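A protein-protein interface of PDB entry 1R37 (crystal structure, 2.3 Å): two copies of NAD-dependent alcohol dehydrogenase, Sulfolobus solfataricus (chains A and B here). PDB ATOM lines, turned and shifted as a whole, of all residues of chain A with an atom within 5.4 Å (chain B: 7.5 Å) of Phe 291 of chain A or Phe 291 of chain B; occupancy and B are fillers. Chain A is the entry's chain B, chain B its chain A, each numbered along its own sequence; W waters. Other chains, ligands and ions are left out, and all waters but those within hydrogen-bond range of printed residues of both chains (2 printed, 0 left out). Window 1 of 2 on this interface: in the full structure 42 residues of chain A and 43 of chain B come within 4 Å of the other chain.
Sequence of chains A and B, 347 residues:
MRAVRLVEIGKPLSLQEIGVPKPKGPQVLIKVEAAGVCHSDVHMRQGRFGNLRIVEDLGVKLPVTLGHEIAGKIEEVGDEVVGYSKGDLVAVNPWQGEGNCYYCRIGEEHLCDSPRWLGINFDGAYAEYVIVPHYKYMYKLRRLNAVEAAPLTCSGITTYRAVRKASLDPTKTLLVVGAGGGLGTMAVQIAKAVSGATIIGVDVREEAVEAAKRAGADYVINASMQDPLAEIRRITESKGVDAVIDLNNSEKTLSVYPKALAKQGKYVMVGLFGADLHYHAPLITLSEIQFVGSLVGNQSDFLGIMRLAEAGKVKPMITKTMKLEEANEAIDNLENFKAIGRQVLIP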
ATOM      1  N   PRO A 258      -4.745 -10.805 -17.105  1.00  0.00           N
ATOM      2  CA  PRO A 258      -5.262 -10.945 -15.736  1.00  0.00           C
ATOM      3  C   PRO A 258      -4.840 -12.285 -15.113  1.00  0.00           C
ATOM      4  O   PRO A 258      -4.698 -12.401 -13.899  1.00  0.00           O
ATOM      5  CB  PRO A 258      -6.769 -10.833 -15.932  1.00  0.00           C
ATOM      6  CG  PRO A 258      -6.860  -9.813 -17.044  1.00  0.00           C
ATOM      7  CD  PRO A 258      -5.787 -10.290 -18.011  1.00  0.00           C
ATOM      8  N   LEU A 261      -1.611 -12.405 -12.873  1.00  0.00           N
ATOM      9  CA  LEU A 261      -1.593 -11.732 -11.573  1.00  0.00           C
ATOM     10  C   LEU A 261      -1.344 -12.654 -10.390  1.00  0.00           C
ATOM     11  O   LEU A 261      -1.889 -13.752 -10.316  1.00  0.00           O
ATOM     12  CB  LEU A 261      -2.916 -11.007 -11.333  1.00  0.00           C
ATOM     13  CG  LEU A 261      -3.326  -9.816 -12.192  1.00  0.00           C
ATOM     14  CD1 LEU A 261      -4.821  -9.578 -12.025  1.00  0.00           C
ATOM     15  CD2 LEU A 261      -2.518  -8.582 -11.791  1.00  0.00           C
ATOM     16  N   TYR A 267      -4.672  -4.910 -11.210  1.00  0.00           N
ATOM     17  CA  TYR A 267      -4.730  -4.726 -12.650  1.00  0.00           C
ATOM     18  C   TYR A 267      -5.229  -3.302 -12.917  1.00  0.00           C
ATOM     19  O   TYR A 267      -6.430  -3.042 -12.914  1.00  0.00           O
ATOM     20  CB  TYR A 267      -5.683  -5.770 -13.255  1.00  0.00           C
ATOM     21  CG  TYR A 267      -5.447  -6.042 -14.722  1.00  0.00           C
ATOM     22  CD1 TYR A 267      -5.965  -5.198 -15.708  1.00  0.00           C
ATOM     23  CD2 TYR A 267      -4.652  -7.117 -15.125  1.00  0.00           C
ATOM     24  CE1 TYR A 267      -5.687  -5.418 -17.066  1.00  0.00           C
ATOM     25  CE2 TYR A 267      -4.366  -7.340 -16.466  1.00  0.00           C
ATOM     26  CZ  TYR A 267      -4.884  -6.488 -17.428  1.00  0.00           C
ATOM     27  OH  TYR A 267      -4.565  -6.703 -18.749  1.00  0.00           O
ATOM     28  N   MET A 269      -6.299  -0.396 -15.033  1.00  0.00           N
ATOM     29  CA  MET A 269      -6.848  -0.284 -16.381  1.00  0.00           C
ATOM     30  C   MET A 269      -6.857   1.144 -16.920  1.00  0.00           C
ATOM     31  O   MET A 269      -7.705   1.958 -16.564  1.00  0.00           O
ATOM     32  CB  MET A 269      -8.257  -0.882 -16.394  1.00  0.00           C
ATOM     33  CG  MET A 269      -8.290  -2.319 -15.879  1.00  0.00           C
ATOM     34  SD  MET A 269      -9.951  -3.010 -15.721  1.00  0.00           S
ATOM     35  CE  MET A 269     -10.496  -2.923 -17.436  1.00  0.00           C
ATOM     36  N   LEU A 277     -14.375  -6.227 -19.731  1.00  0.00           N
ATOM     37  CA  LEU A 277     -13.641  -7.028 -18.764  1.00  0.00           C
ATOM     38  C   LEU A 277     -14.533  -8.221 -18.442  1.00  0.00           C
ATOM     39  O   LEU A 277     -15.732  -8.061 -18.212  1.00  0.00           O
ATOM     40  CB  LEU A 277     -13.364  -6.222 -17.497  1.00  0.00           C
ATOM     41  CG  LEU A 277     -12.875  -7.046 -16.305  1.00  0.00           C
ATOM     42  CD1 LEU A 277     -11.526  -7.674 -16.638  1.00  0.00           C
ATOM     43  CD2 LEU A 277     -12.779  -6.165 -15.067  1.00  0.00           C
ATOM     44  N   TYR A 279     -14.183 -11.806 -16.099  1.00  0.00           N
ATOM     45  CA  TYR A 279     -13.377 -12.653 -15.230  1.00  0.00           C
ATOM     46  C   TYR A 279     -14.244 -13.348 -14.180  1.00  0.00           C
ATOM     47  O   TYR A 279     -15.154 -12.739 -13.617  1.00  0.00           O
ATOM     48  CB  TYR A 279     -12.302 -11.796 -14.546  1.00  0.00           C
ATOM     49  CG  TYR A 279     -11.005 -12.529 -14.300  1.00  0.00           C
ATOM     50  CD1 TYR A 279     -10.564 -12.794 -13.008  1.00  0.00           C
ATOM     51  CD2 TYR A 279     -10.234 -12.991 -15.367  1.00  0.00           C
ATOM     52  CE1 TYR A 279      -9.390 -13.503 -12.783  1.00  0.00           C
ATOM     53  CE2 TYR A 279      -9.064 -13.699 -15.154  1.00  0.00           C
ATOM     54  CZ  TYR A 279      -8.649 -13.954 -13.861  1.00  0.00           C
ATOM     55  OH  TYR A 279      -7.498 -14.671 -13.651  1.00  0.00           O
ATOM     56  N   ILE A 284     -11.605 -13.865  -8.449  1.00  0.00           N
ATOM     57  CA  ILE A 284     -11.226 -12.539  -7.992  1.00  0.00           C
ATOM     58  C   ILE A 284     -11.189 -12.547  -6.463  1.00  0.00           C
ATOM     59  O   ILE A 284     -10.226 -12.090  -5.844  1.00  0.00           O
ATOM     60  CB  ILE A 284     -12.244 -11.465  -8.468  1.00  0.00           C
ATOM     61  CG1 ILE A 284     -12.179 -11.319  -9.997  1.00  0.00           C
ATOM     62  CG2 ILE A 284     -11.965 -10.139  -7.777  1.00  0.00           C
ATOM     63  CD1 ILE A 284     -13.232 -10.412 -10.574  1.00  0.00           C
ATOM     64  N   ILE A 289      -7.587 -10.276  -6.041  1.00  0.00           N
ATOM     65  CA  ILE A 289      -7.062  -9.381  -7.056  1.00  0.00           C
ATOM     66  C   ILE A 289      -8.015  -8.209  -7.190  1.00  0.00           C
ATOM     67  O   ILE A 289      -9.143  -8.254  -6.685  1.00  0.00           O
ATOM     68  CB  ILE A 289      -6.868 -10.075  -8.434  1.00  0.00           C
ATOM     69  CG1 ILE A 289      -8.178 -10.689  -8.921  1.00  0.00           C
ATOM     70  CG2 ILE A 289      -5.771 -11.115  -8.336  1.00  0.00           C
ATOM     71  CD1 ILE A 289      -8.045 -11.401 -10.260  1.00  0.00           C
ATOM     72  N   GLN A 290      -7.546  -7.148  -7.838  1.00  0.00           N
ATOM     73  CA  GLN A 290      -8.356  -5.962  -8.042  1.00  0.00           C
ATOM     74  C   GLN A 290      -8.216  -5.475  -9.477  1.00  0.00           C
ATOM     75  O   GLN A 290      -7.158  -5.607 -10.093  1.00  0.00           O
ATOM     76  CB  GLN A 290      -7.915  -4.825  -7.111  1.00  0.00           C
ATOM     77  CG  GLN A 290      -7.212  -5.258  -5.831  1.00  0.00           C
ATOM     78  CD  GLN A 290      -7.064  -4.103  -4.844  1.00  0.00           C
ATOM     79  OE1 GLN A 290      -6.938  -2.943  -5.242  1.00  0.00           O
ATOM     80  NE2 GLN A 290      -7.075  -4.419  -3.551  1.00  0.00           N
ATOM     81  N   PHE A 291      -9.300  -4.923  -9.999  1.00  0.00           N
ATOM     82  CA  PHE A 291      -9.304  -4.329 -11.320  1.00  0.00           C
ATOM     83  C   PHE A 291      -9.629  -2.880 -11.014  1.00  0.00           C
ATOM     84  O   PHE A 291     -10.746  -2.568 -10.608  1.00  0.00           O
ATOM     85  CB  PHE A 291     -10.393  -4.961 -12.190  1.00  0.00           C
ATOM     86  CG  PHE A 291     -10.089  -6.382 -12.608  1.00  0.00           C
ATOM     87  CD1 PHE A 291      -9.241  -6.642 -13.675  1.00  0.00           C
ATOM     88  CD2 PHE A 291     -10.636  -7.456 -11.919  1.00  0.00           C
ATOM     89  CE1 PHE A 291      -8.943  -7.949 -14.053  1.00  0.00           C
ATOM     90  CE2 PHE A 291     -10.344  -8.768 -12.289  1.00  0.00           C
ATOM     91  CZ  PHE A 291      -9.496  -9.012 -13.359  1.00  0.00           C
ATOM     92  N   VAL A 292      -8.649  -1.995 -11.175  1.00  0.00           N
ATOM     93  CA  VAL A 292      -8.880  -0.599 -10.844  1.00  0.00           C
ATOM     94  C   VAL A 292      -8.684   0.341 -12.026  1.00  0.00           C
ATOM     95  O   VAL A 292      -7.663   0.305 -12.709  1.00  0.00           O
ATOM     96  CB  VAL A 292      -7.964  -0.145  -9.660  1.00  0.00           C
ATOM     97  CG1 VAL A 292      -7.751  -1.307  -8.682  1.00  0.00           C
ATOM     98  CG2 VAL A 292      -6.644   0.371 -10.172  1.00  0.00           C
ATOM     99  N   GLY A 293      -9.680   1.182 -12.270  1.00  0.00           N
ATOM    100  CA  GLY A 293      -9.570   2.133 -13.355  1.00  0.00           C
ATOM    101  C   GLY A 293      -8.776   3.344 -12.910  1.00  0.00           C
ATOM    102  O   GLY A 293      -8.840   3.749 -11.745  1.00  0.00           O
ATOM    103  N   ASN B 249     -22.410 -11.961  -5.378  1.00  0.00           N
ATOM    104  CA  ASN B 249     -21.614 -12.015  -6.603  1.00  0.00           C
ATOM    105  C   ASN B 249     -22.194 -13.057  -7.560  1.00  0.00           C
ATOM    106  O   ASN B 249     -21.478 -13.907  -8.101  1.00  0.00           O
ATOM    107  CB  ASN B 249     -20.143 -12.308  -6.284  1.00  0.00           C
ATOM    108  CG  ASN B 249     -19.417 -11.086  -5.727  1.00  0.00           C
ATOM    109  OD1 ASN B 249     -18.644 -11.180  -4.773  1.00  0.00           O
ATOM    110  ND2 ASN B 249     -19.666  -9.932  -6.330  1.00  0.00           N
ATOM    111  N   LEU B 254     -24.254  -8.948  -9.822  1.00  0.00           N
ATOM    112  CA  LEU B 254     -23.212  -8.371 -10.671  1.00  0.00           C
ATOM    113  C   LEU B 254     -23.708  -7.639 -11.910  1.00  0.00           C
ATOM    114  O   LEU B 254     -23.003  -6.792 -12.455  1.00  0.00           O
ATOM    115  CB  LEU B 254     -22.204  -9.451 -11.098  1.00  0.00           C
ATOM    116  CG  LEU B 254     -21.219  -9.896 -10.007  1.00  0.00           C
ATOM    117  CD1 LEU B 254     -20.271 -10.949 -10.561  1.00  0.00           C
ATOM    118  CD2 LEU B 254     -20.439  -8.692  -9.501  1.00  0.00           C
ATOM    119  N   TYR B 257     -25.828  -4.002  -9.434  1.00  0.00           N
ATOM    120  CA  TYR B 257     -25.207  -3.032  -8.546  1.00  0.00           C
ATOM    121  C   TYR B 257     -23.973  -2.258  -8.997  1.00  0.00           C
ATOM    122  O   TYR B 257     -23.772  -1.140  -8.550  1.00  0.00           O
ATOM    123  CB  TYR B 257     -25.002  -3.685  -7.184  1.00  0.00           C
ATOM    124  CG  TYR B 257     -26.340  -4.097  -6.607  1.00  0.00           C
ATOM    125  CD1 TYR B 257     -27.295  -3.132  -6.262  1.00  0.00           C
ATOM    126  CD2 TYR B 257     -26.697  -5.440  -6.502  1.00  0.00           C
ATOM    127  CE1 TYR B 257     -28.572  -3.498  -5.835  1.00  0.00           C
ATOM    128  CE2 TYR B 257     -27.978  -5.817  -6.075  1.00  0.00           C
ATOM    129  CZ  TYR B 257     -28.906  -4.842  -5.747  1.00  0.00           C
ATOM    130  OH  TYR B 257     -30.168  -5.208  -5.340  1.00  0.00           O
ATOM    131  N   PRO B 258     -23.137  -2.821  -9.889  1.00  0.00           N
ATOM    132  CA  PRO B 258     -21.976  -2.019 -10.297  1.00  0.00           C
ATOM    133  C   PRO B 258     -22.422  -0.695 -10.936  1.00  0.00           C
ATOM    134  O   PRO B 258     -21.704   0.300 -10.890  1.00  0.00           O
ATOM    135  CB  PRO B 258     -21.254  -2.931 -11.286  1.00  0.00           C
ATOM    136  CG  PRO B 258     -21.588  -4.317 -10.767  1.00  0.00           C
ATOM    137  CD  PRO B 258     -23.061  -4.183 -10.451  1.00  0.00           C
ATOM    138  N   LYS B 259     -23.623  -0.689 -11.509  1.00  0.00           N
ATOM    139  CA  LYS B 259     -24.178   0.505 -12.144  1.00  0.00           C
ATOM    140  C   LYS B 259     -24.566   1.569 -11.122  1.00  0.00           C
ATOM    141  O   LYS B 259     -24.852   2.707 -11.483  1.00  0.00           O
ATOM    142  CB  LYS B 259     -25.417   0.138 -12.970  1.00  0.00           C
ATOM    143  CG  LYS B 259     -25.145  -0.847 -14.091  1.00  0.00           C
ATOM    144  CD  LYS B 259     -26.428  -1.260 -14.794  1.00  0.00           C
ATOM    145  CE  LYS B 259     -26.116  -2.084 -16.035  1.00  0.00           C
ATOM    146  NZ  LYS B 259     -27.345  -2.645 -16.669  1.00  0.00           N
ATOM    147  N   LEU B 261     -22.562   2.479  -8.671  1.00  0.00           N
ATOM    148  CA  LEU B 261     -21.315   3.036  -8.156  1.00  0.00           C
ATOM    149  C   LEU B 261     -21.081   4.481  -8.554  1.00  0.00           C
ATOM    150  O   LEU B 261     -21.352   4.877  -9.686  1.00  0.00           O
ATOM    151  CB  LEU B 261     -20.115   2.210  -8.643  1.00  0.00           C
ATOM    152  CG  LEU B 261     -19.853   0.825  -8.062  1.00  0.00           C
ATOM    153  CD1 LEU B 261     -18.686   0.187  -8.793  1.00  0.00           C
ATOM    154  CD2 LEU B 261     -19.553   0.938  -6.572  1.00  0.00           C
ATOM    155  N   GLY B 265     -15.894   4.653  -6.988  1.00  0.00           N
ATOM    156  CA  GLY B 265     -16.545   3.638  -6.174  1.00  0.00           C
ATOM    157  C   GLY B 265     -15.815   2.312  -6.091  1.00  0.00           C
ATOM    158  O   GLY B 265     -15.230   1.848  -7.068  1.00  0.00           O
ATOM    159  N   LYS B 266     -15.850   1.694  -4.915  1.00  0.00           N
ATOM    160  CA  LYS B 266     -15.200   0.406  -4.722  1.00  0.00           C
ATOM    161  C   LYS B 266     -16.214  -0.707  -4.555  1.00  0.00           C
ATOM    162  O   LYS B 266     -17.035  -0.684  -3.639  1.00  0.00           O
ATOM    163  CB  LYS B 266     -14.271   0.458  -3.510  1.00  0.00           C
ATOM    164  CG  LYS B 266     -13.156   1.480  -3.688  1.00  0.00           C
ATOM    165  CD  LYS B 266     -12.287   1.632  -2.450  1.00  0.00           C
ATOM    166  CE  LYS B 266     -11.281   2.747  -2.668  1.00  0.00           C
ATOM    167  NZ  LYS B 266     -11.982   3.981  -3.161  1.00  0.00           N
ATOM    168  N   TYR B 267     -16.153  -1.677  -5.459  1.00  0.00           N
ATOM    169  CA  TYR B 267     -17.046  -2.820  -5.427  1.00  0.00           C
ATOM    170  C   TYR B 267     -16.279  -3.978  -4.789  1.00  0.00           C
ATOM    171  O   TYR B 267     -15.469  -4.639  -5.443  1.00  0.00           O
ATOM    172  CB  TYR B 267     -17.491  -3.159  -6.858  1.00  0.00           C
ATOM    173  CG  TYR B 267     -18.775  -3.949  -6.931  1.00  0.00           C
ATOM    174  CD1 TYR B 267     -18.779  -5.333  -6.759  1.00  0.00           C
ATOM    175  CD2 TYR B 267     -20.003  -3.305  -7.126  1.00  0.00           C
ATOM    176  CE1 TYR B 267     -19.969  -6.056  -6.778  1.00  0.00           C
ATOM    177  CE2 TYR B 267     -21.196  -4.023  -7.139  1.00  0.00           C
ATOM    178  CZ  TYR B 267     -21.170  -5.395  -6.963  1.00  0.00           C
ATOM    179  OH  TYR B 267     -22.350  -6.102  -6.958  1.00  0.00           O
ATOM    180  N   VAL B 268     -16.527  -4.209  -3.502  1.00  0.00           N
ATOM    181  CA  VAL B 268     -15.837  -5.260  -2.763  1.00  0.00           C
ATOM    182  C   VAL B 268     -16.577  -6.576  -2.980  1.00  0.00           C
ATOM    183  O   VAL B 268     -17.745  -6.706  -2.614  1.00  0.00           O
ATOM    184  CB  VAL B 268     -15.772  -4.923  -1.263  1.00  0.00           C
ATOM    185  CG1 VAL B 268     -14.851  -5.894  -0.548  1.00  0.00           C
ATOM    186  CG2 VAL B 268     -15.273  -3.489  -1.078  1.00  0.00           C
ATOM    187  N   MET B 269     -15.887  -7.545  -3.579  1.00  0.00           N
ATOM    188  CA  MET B 269     -16.488  -8.826  -3.927  1.00  0.00           C
ATOM    189  C   MET B 269     -16.171  -9.936  -2.922  1.00  0.00           C
ATOM    190  O   MET B 269     -15.074 -10.500  -2.905  1.00  0.00           O
ATOM    191  CB  MET B 269     -16.040  -9.208  -5.346  1.00  0.00           C
ATOM    192  CG  MET B 269     -16.407  -8.138  -6.380  1.00  0.00           C
ATOM    193  SD  MET B 269     -15.793  -8.432  -8.053  1.00  0.00           S
ATOM    194  CE  MET B 269     -16.673  -9.958  -8.441  1.00  0.00           C
ATOM    195  N   LEU B 277     -17.780 -11.686 -13.500  1.00  0.00           N
ATOM    196  CA  LEU B 277     -17.854 -10.236 -13.540  1.00  0.00           C
ATOM    197  C   LEU B 277     -17.755  -9.846 -15.015  1.00  0.00           C
ATOM    198  O   LEU B 277     -16.894 -10.346 -15.738  1.00  0.00           O
ATOM    199  CB  LEU B 277     -16.690  -9.618 -12.771  1.00  0.00           C
ATOM    200  CG  LEU B 277     -16.589  -8.098 -12.921  1.00  0.00           C
ATOM    201  CD1 LEU B 277     -17.761  -7.451 -12.191  1.00  0.00           C
ATOM    202  CD2 LEU B 277     -15.264  -7.599 -12.364  1.00  0.00           C
ATOM    203  N   HIS B 278     -18.639  -8.962 -15.459  1.00  0.00           N
ATOM    204  CA  HIS B 278     -18.644  -8.527 -16.849  1.00  0.00           C
ATOM    205  C   HIS B 278     -19.048  -7.059 -16.882  1.00  0.00           C
ATOM    206  O   HIS B 278     -20.184  -6.708 -16.553  1.00  0.00           O
ATOM    207  CB  HIS B 278     -19.619  -9.388 -17.655  1.00  0.00           C
ATOM    208  CG  HIS B 278     -19.602  -9.110 -19.125  1.00  0.00           C
ATOM    209  ND1 HIS B 278     -20.157  -7.974 -19.676  1.00  0.00           N
ATOM    210  CD2 HIS B 278     -19.080  -9.813 -20.159  1.00  0.00           C
ATOM    211  CE1 HIS B 278     -19.978  -7.989 -20.985  1.00  0.00           C
ATOM    212  NE2 HIS B 278     -19.327  -9.093 -21.304  1.00  0.00           N
ATOM    213  N   TYR B 279     -18.105  -6.202 -17.264  1.00  0.00           N
ATOM    214  CA  TYR B 279     -18.348  -4.767 -17.291  1.00  0.00           C
ATOM    215  C   TYR B 279     -17.480  -4.117 -18.367  1.00  0.00           C
ATOM    216  O   TYR B 279     -16.327  -4.500 -18.560  1.00  0.00           O
ATOM    217  CB  TYR B 279     -18.025  -4.176 -15.913  1.00  0.00           C
ATOM    218  CG  TYR B 279     -18.872  -2.986 -15.536  1.00  0.00           C
ATOM    219  CD1 TYR B 279     -18.308  -1.721 -15.395  1.00  0.00           C
ATOM    220  CD2 TYR B 279     -20.243  -3.125 -15.326  1.00  0.00           C
ATOM    221  CE1 TYR B 279     -19.088  -0.619 -15.053  1.00  0.00           C
ATOM    222  CE2 TYR B 279     -21.032  -2.031 -14.985  1.00  0.00           C
ATOM    223  CZ  TYR B 279     -20.446  -0.782 -14.851  1.00  0.00           C
ATOM    224  OH  TYR B 279     -21.220   0.303 -14.513  1.00  0.00           O
ATOM    225  N   HIS B 280     -18.044  -3.134 -19.065  1.00  0.00           N
ATOM    226  CA  HIS B 280     -17.335  -2.445 -20.140  1.00  0.00           C
ATOM    227  C   HIS B 280     -16.124  -1.692 -19.575  1.00  0.00           C
ATOM    228  O   HIS B 280     -16.273  -0.785 -18.759  1.00  0.00           O
ATOM    229  CB  HIS B 280     -18.302  -1.491 -20.862  1.00  0.00           C
ATOM    230  CG  HIS B 280     -17.822  -1.038 -22.208  1.00  0.00           C
ATOM    231  ND1 HIS B 280     -17.329  -1.909 -23.156  1.00  0.00           N
ATOM    232  CD2 HIS B 280     -17.777   0.194 -22.771  1.00  0.00           C
ATOM    233  CE1 HIS B 280     -17.000  -1.234 -24.243  1.00  0.00           C
ATOM    234  NE2 HIS B 280     -17.262   0.045 -24.036  1.00  0.00           N
ATOM    235  N   LEU B 283     -15.701   2.101 -19.165  1.00  0.00           N
ATOM    236  CA  LEU B 283     -16.560   2.603 -18.096  1.00  0.00           C
ATOM    237  C   LEU B 283     -15.829   2.531 -16.753  1.00  0.00           C
ATOM    238  O   LEU B 283     -16.003   3.390 -15.890  1.00  0.00           O
ATOM    239  CB  LEU B 283     -17.846   1.770 -18.063  1.00  0.00           C
ATOM    240  CG  LEU B 283     -19.169   2.413 -17.632  1.00  0.00           C
ATOM    241  CD1 LEU B 283     -19.297   3.823 -18.190  1.00  0.00           C
ATOM    242  CD2 LEU B 283     -20.318   1.534 -18.129  1.00  0.00           C
ATOM    243  N   ILE B 284     -15.011   1.496 -16.587  1.00  0.00           N
ATOM    244  CA  ILE B 284     -14.227   1.325 -15.369  1.00  0.00           C
ATOM    245  C   ILE B 284     -13.181   2.435 -15.325  1.00  0.00           C
ATOM    246  O   ILE B 284     -13.043   3.138 -14.331  1.00  0.00           O
ATOM    247  CB  ILE B 284     -13.505  -0.058 -15.351  1.00  0.00           C
ATOM    248  CG1 ILE B 284     -14.537  -1.190 -15.391  1.00  0.00           C
ATOM    249  CG2 ILE B 284     -12.634  -0.176 -14.111  1.00  0.00           C
ATOM    250  CD1 ILE B 284     -13.948  -2.576 -15.336  1.00  0.00           C
ATOM    251  N   GLU B 288     -13.064   5.515 -12.802  1.00  0.00           N
ATOM    252  CA  GLU B 288     -12.076   5.069 -11.817  1.00  0.00           C
ATOM    253  C   GLU B 288     -12.679   4.136 -10.771  1.00  0.00           C
ATOM    254  O   GLU B 288     -12.285   4.185  -9.600  1.00  0.00           O
ATOM    255  CB  GLU B 288     -11.424   6.250 -11.081  1.00  0.00           C
ATOM    256  CG  GLU B 288     -10.473   7.090 -11.916  1.00  0.00           C
ATOM    257  CD  GLU B 288      -9.442   7.806 -11.057  1.00  0.00           C
ATOM    258  OE1 GLU B 288      -9.765   8.155  -9.902  1.00  0.00           O
ATOM    259  OE2 GLU B 288      -8.308   8.025 -11.534  1.00  0.00           O
ATOM    260  N   ILE B 289     -13.631   3.294 -11.167  1.00  0.00           N
ATOM    261  CA  ILE B 289     -14.194   2.368 -10.194  1.00  0.00           C
ATOM    262  C   ILE B 289     -13.232   1.208 -10.051  1.00  0.00           C
ATOM    263  O   ILE B 289     -12.345   1.026 -10.889  1.00  0.00           O
ATOM    264  CB  ILE B 289     -15.599   1.824 -10.601  1.00  0.00           C
ATOM    265  CG1 ILE B 289     -15.537   1.128 -11.953  1.00  0.00           C
ATOM    266  CG2 ILE B 289     -16.624   2.957 -10.605  1.00  0.00           C
ATOM    267  CD1 ILE B 289     -16.894   0.600 -12.414  1.00  0.00           C
ATOM    268  N   GLN B 290     -13.399   0.444  -8.978  1.00  0.00           N
ATOM    269  CA  GLN B 290     -12.547  -0.703  -8.723  1.00  0.00           C
ATOM    270  C   GLN B 290     -13.402  -1.899  -8.343  1.00  0.00           C
ATOM    271  O   GLN B 290     -14.464  -1.755  -7.735  1.00  0.00           O
ATOM    272  CB  GLN B 290     -11.582  -0.427  -7.564  1.00  0.00           C
ATOM    273  CG  GLN B 290     -11.200   1.028  -7.365  1.00  0.00           C
ATOM    274  CD  GLN B 290     -10.066   1.196  -6.358  1.00  0.00           C
ATOM    275  OE1 GLN B 290      -9.946   0.426  -5.403  1.00  0.00           O
ATOM    276  NE2 GLN B 290      -9.234   2.211  -6.569  1.00  0.00           N
ATOM    277  N   PHE B 291     -12.928  -3.079  -8.711  1.00  0.00           N
ATOM    278  CA  PHE B 291     -13.589  -4.316  -8.337  1.00  0.00           C
ATOM    279  C   PHE B 291     -12.504  -5.013  -7.536  1.00  0.00           C
ATOM    280  O   PHE B 291     -11.478  -5.415  -8.098  1.00  0.00           O
ATOM    281  CB  PHE B 291     -13.958  -5.131  -9.581  1.00  0.00           C
ATOM    282  CG  PHE B 291     -15.066  -4.515 -10.405  1.00  0.00           C
ATOM    283  CD1 PHE B 291     -16.393  -4.670 -10.034  1.00  0.00           C
ATOM    284  CD2 PHE B 291     -14.776  -3.783 -11.546  1.00  0.00           C
ATOM    285  CE1 PHE B 291     -17.414  -4.108 -10.784  1.00  0.00           C
ATOM    286  CE2 PHE B 291     -15.795  -3.213 -12.305  1.00  0.00           C
ATOM    287  CZ  PHE B 291     -17.113  -3.377 -11.924  1.00  0.00           C
ATOM    288  N   VAL B 292     -12.714  -5.134  -6.227  1.00  0.00           N
ATOM    289  CA  VAL B 292     -11.703  -5.726  -5.369  1.00  0.00           C
ATOM    290  C   VAL B 292     -12.174  -6.964  -4.609  1.00  0.00           C
ATOM    291  O   VAL B 292     -13.202  -6.945  -3.936  1.00  0.00           O
ATOM    292  CB  VAL B 292     -11.165  -4.676  -4.354  1.00  0.00           C
ATOM    293  CG1 VAL B 292     -11.023  -3.316  -5.040  1.00  0.00           C
ATOM    294  CG2 VAL B 292     -12.083  -4.570  -3.160  1.00  0.00           C
ATOM    295  N   GLY B 293     -11.412  -8.043  -4.725  1.00  0.00           N
ATOM    296  CA  GLY B 293     -11.758  -9.259  -4.020  1.00  0.00           C
ATOM    297  C   GLY B 293     -11.282  -9.189  -2.581  1.00  0.00           C
ATOM    298  O   GLY B 293     -10.237  -8.609  -2.284  1.00  0.00           O
HETATM  299  O   HOH W   1      -8.120  -6.870  -3.033  1.00  0.00           O
HETATM  300  O   HOH W   2      -9.521   3.646  -8.886  1.00  0.00           O
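Water W1 lies within hydrogen-bond range of the side-chain amide nitrogen (NE2) of Gln 290 of chain A (2.7 Å) and the backbone carbonyl oxygen (O) of Gly 293 of chain B (2.8 Å).
Water W2 lies within hydrogen-bond range of the side-chain amide nitrogen (NE2) of Gln 290 of chain B (2.7 Å), the backbone carbonyl oxygen (O) of Glu 288 of chain B (2.9 Å) and the backbone carbonyl oxygen (O) of Gly 293 of chain A (2.9 Å).
Ile 289 of chain A touches Val 292 of chain B, and with the chains exchanged Val 292 of chain A touches Ile 289 of chain B.
Phe 291 of chain A touches its own counterpart, Phe 291 of chain B.
Positions printed for both chains: 258, 261, 267, 269, 277, 279, 284, 289, 290, 291, 292 and 293.
Of the printed residues of chain B, Tyr 279 of chain A touches Leu 277.
Phe 291 of chain A touches just these residues of chain B: Ile 289 (3.9 Å), Gln 290 (3.2 Å) and Phe 291 (2.9 Å).
Leu 261 of chain B touches none of the printed residues of chain A.
Of the printed residues of chain A, Leu 277 of chain B touches Leu 277, Tyr 279 and Ile 284.
Of the printed residues of chain A, Phe 291 of chain B touches Ile 289 (3.9 Å), Gln 290 (3.2 Å) and Phe 291 (2.9 Å).
The nearest printed residue of chain B that does not touch Phe 291 of chain A is Ile 284 of chain B (4.6 Å).
The nearest residue of chain A that does not touch Phe 291 of chain B is Leu 277 of chain A (4.7 Å).
The nearest printed residue of chain B that does not touch Gln 290 of chain A is Val 292 of chain B (4.03 Å).
Ile 284 of chain A touches Leu 277 of chain B (CD1 to CD2, 3.9 Å).
Ile 284 of chain A touches Gly 293 of chain B (O to CA, 3.7 Å).
O of Phe 291 of chain B touches O of Ile 289 of chain A, 3.9 Å away.
CA of Gln 290 of chain A touches O of Phe 291 of chain B, 3.2 Å away.
CG2 of Ile 284 of chain B touches N of Gly 293 of chain A, 3.7 Å away.
CA of Glu 288 of chain B touches O of Gly 293 of chain A, at 3.5 Å.
The backbone carbonyl oxygen (O) of Ile 289 of chain A is in hydrogen-bond range of the backbone NH (N) of Gly 293 of chain B (3.0 Å).
O of Phe 291 of chain B lies within hydrogen-bond range of N of Phe 291 of chain A.
The backbone carbonyl oxygen (O) of Tyr 279 of chain A is in hydrogen-bond range of the backbone NH (N) of Leu 277 of chain B (2.8 Å).
O of Ile 289 of chain B sits at hydrogen-bond distance from N of Gly 293 of chain A, at 3.0 Å.
The backbone carbonyl oxygen (O) of Tyr 279 of chain B lies within hydrogen-bond range of the backbone NH (N) of Leu 277 of chain A, at 2.9 Å.
The backbone NH of Tyr 267 of chain B sits at hydrogen-bond distance from the backbone carbonyl oxygen of Gln 290 of chain B (2.8 Å).
N of Gln 290 of chain B lies within hydrogen-bond range of O of Gly 265 of chain B (3.0 Å).
N of Ile 289 of chain A is in hydrogen-bond range of O of Ile 284 of chain A (3.2 Å).
N of Met 269 of chain A sits at hydrogen-bond distance from O of Val 292 of chain A, at 2.8 Å.
Hydrophobic or aromatic side chains of chain B that line the printed part of chain A: Leu 277 and Ile 284.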
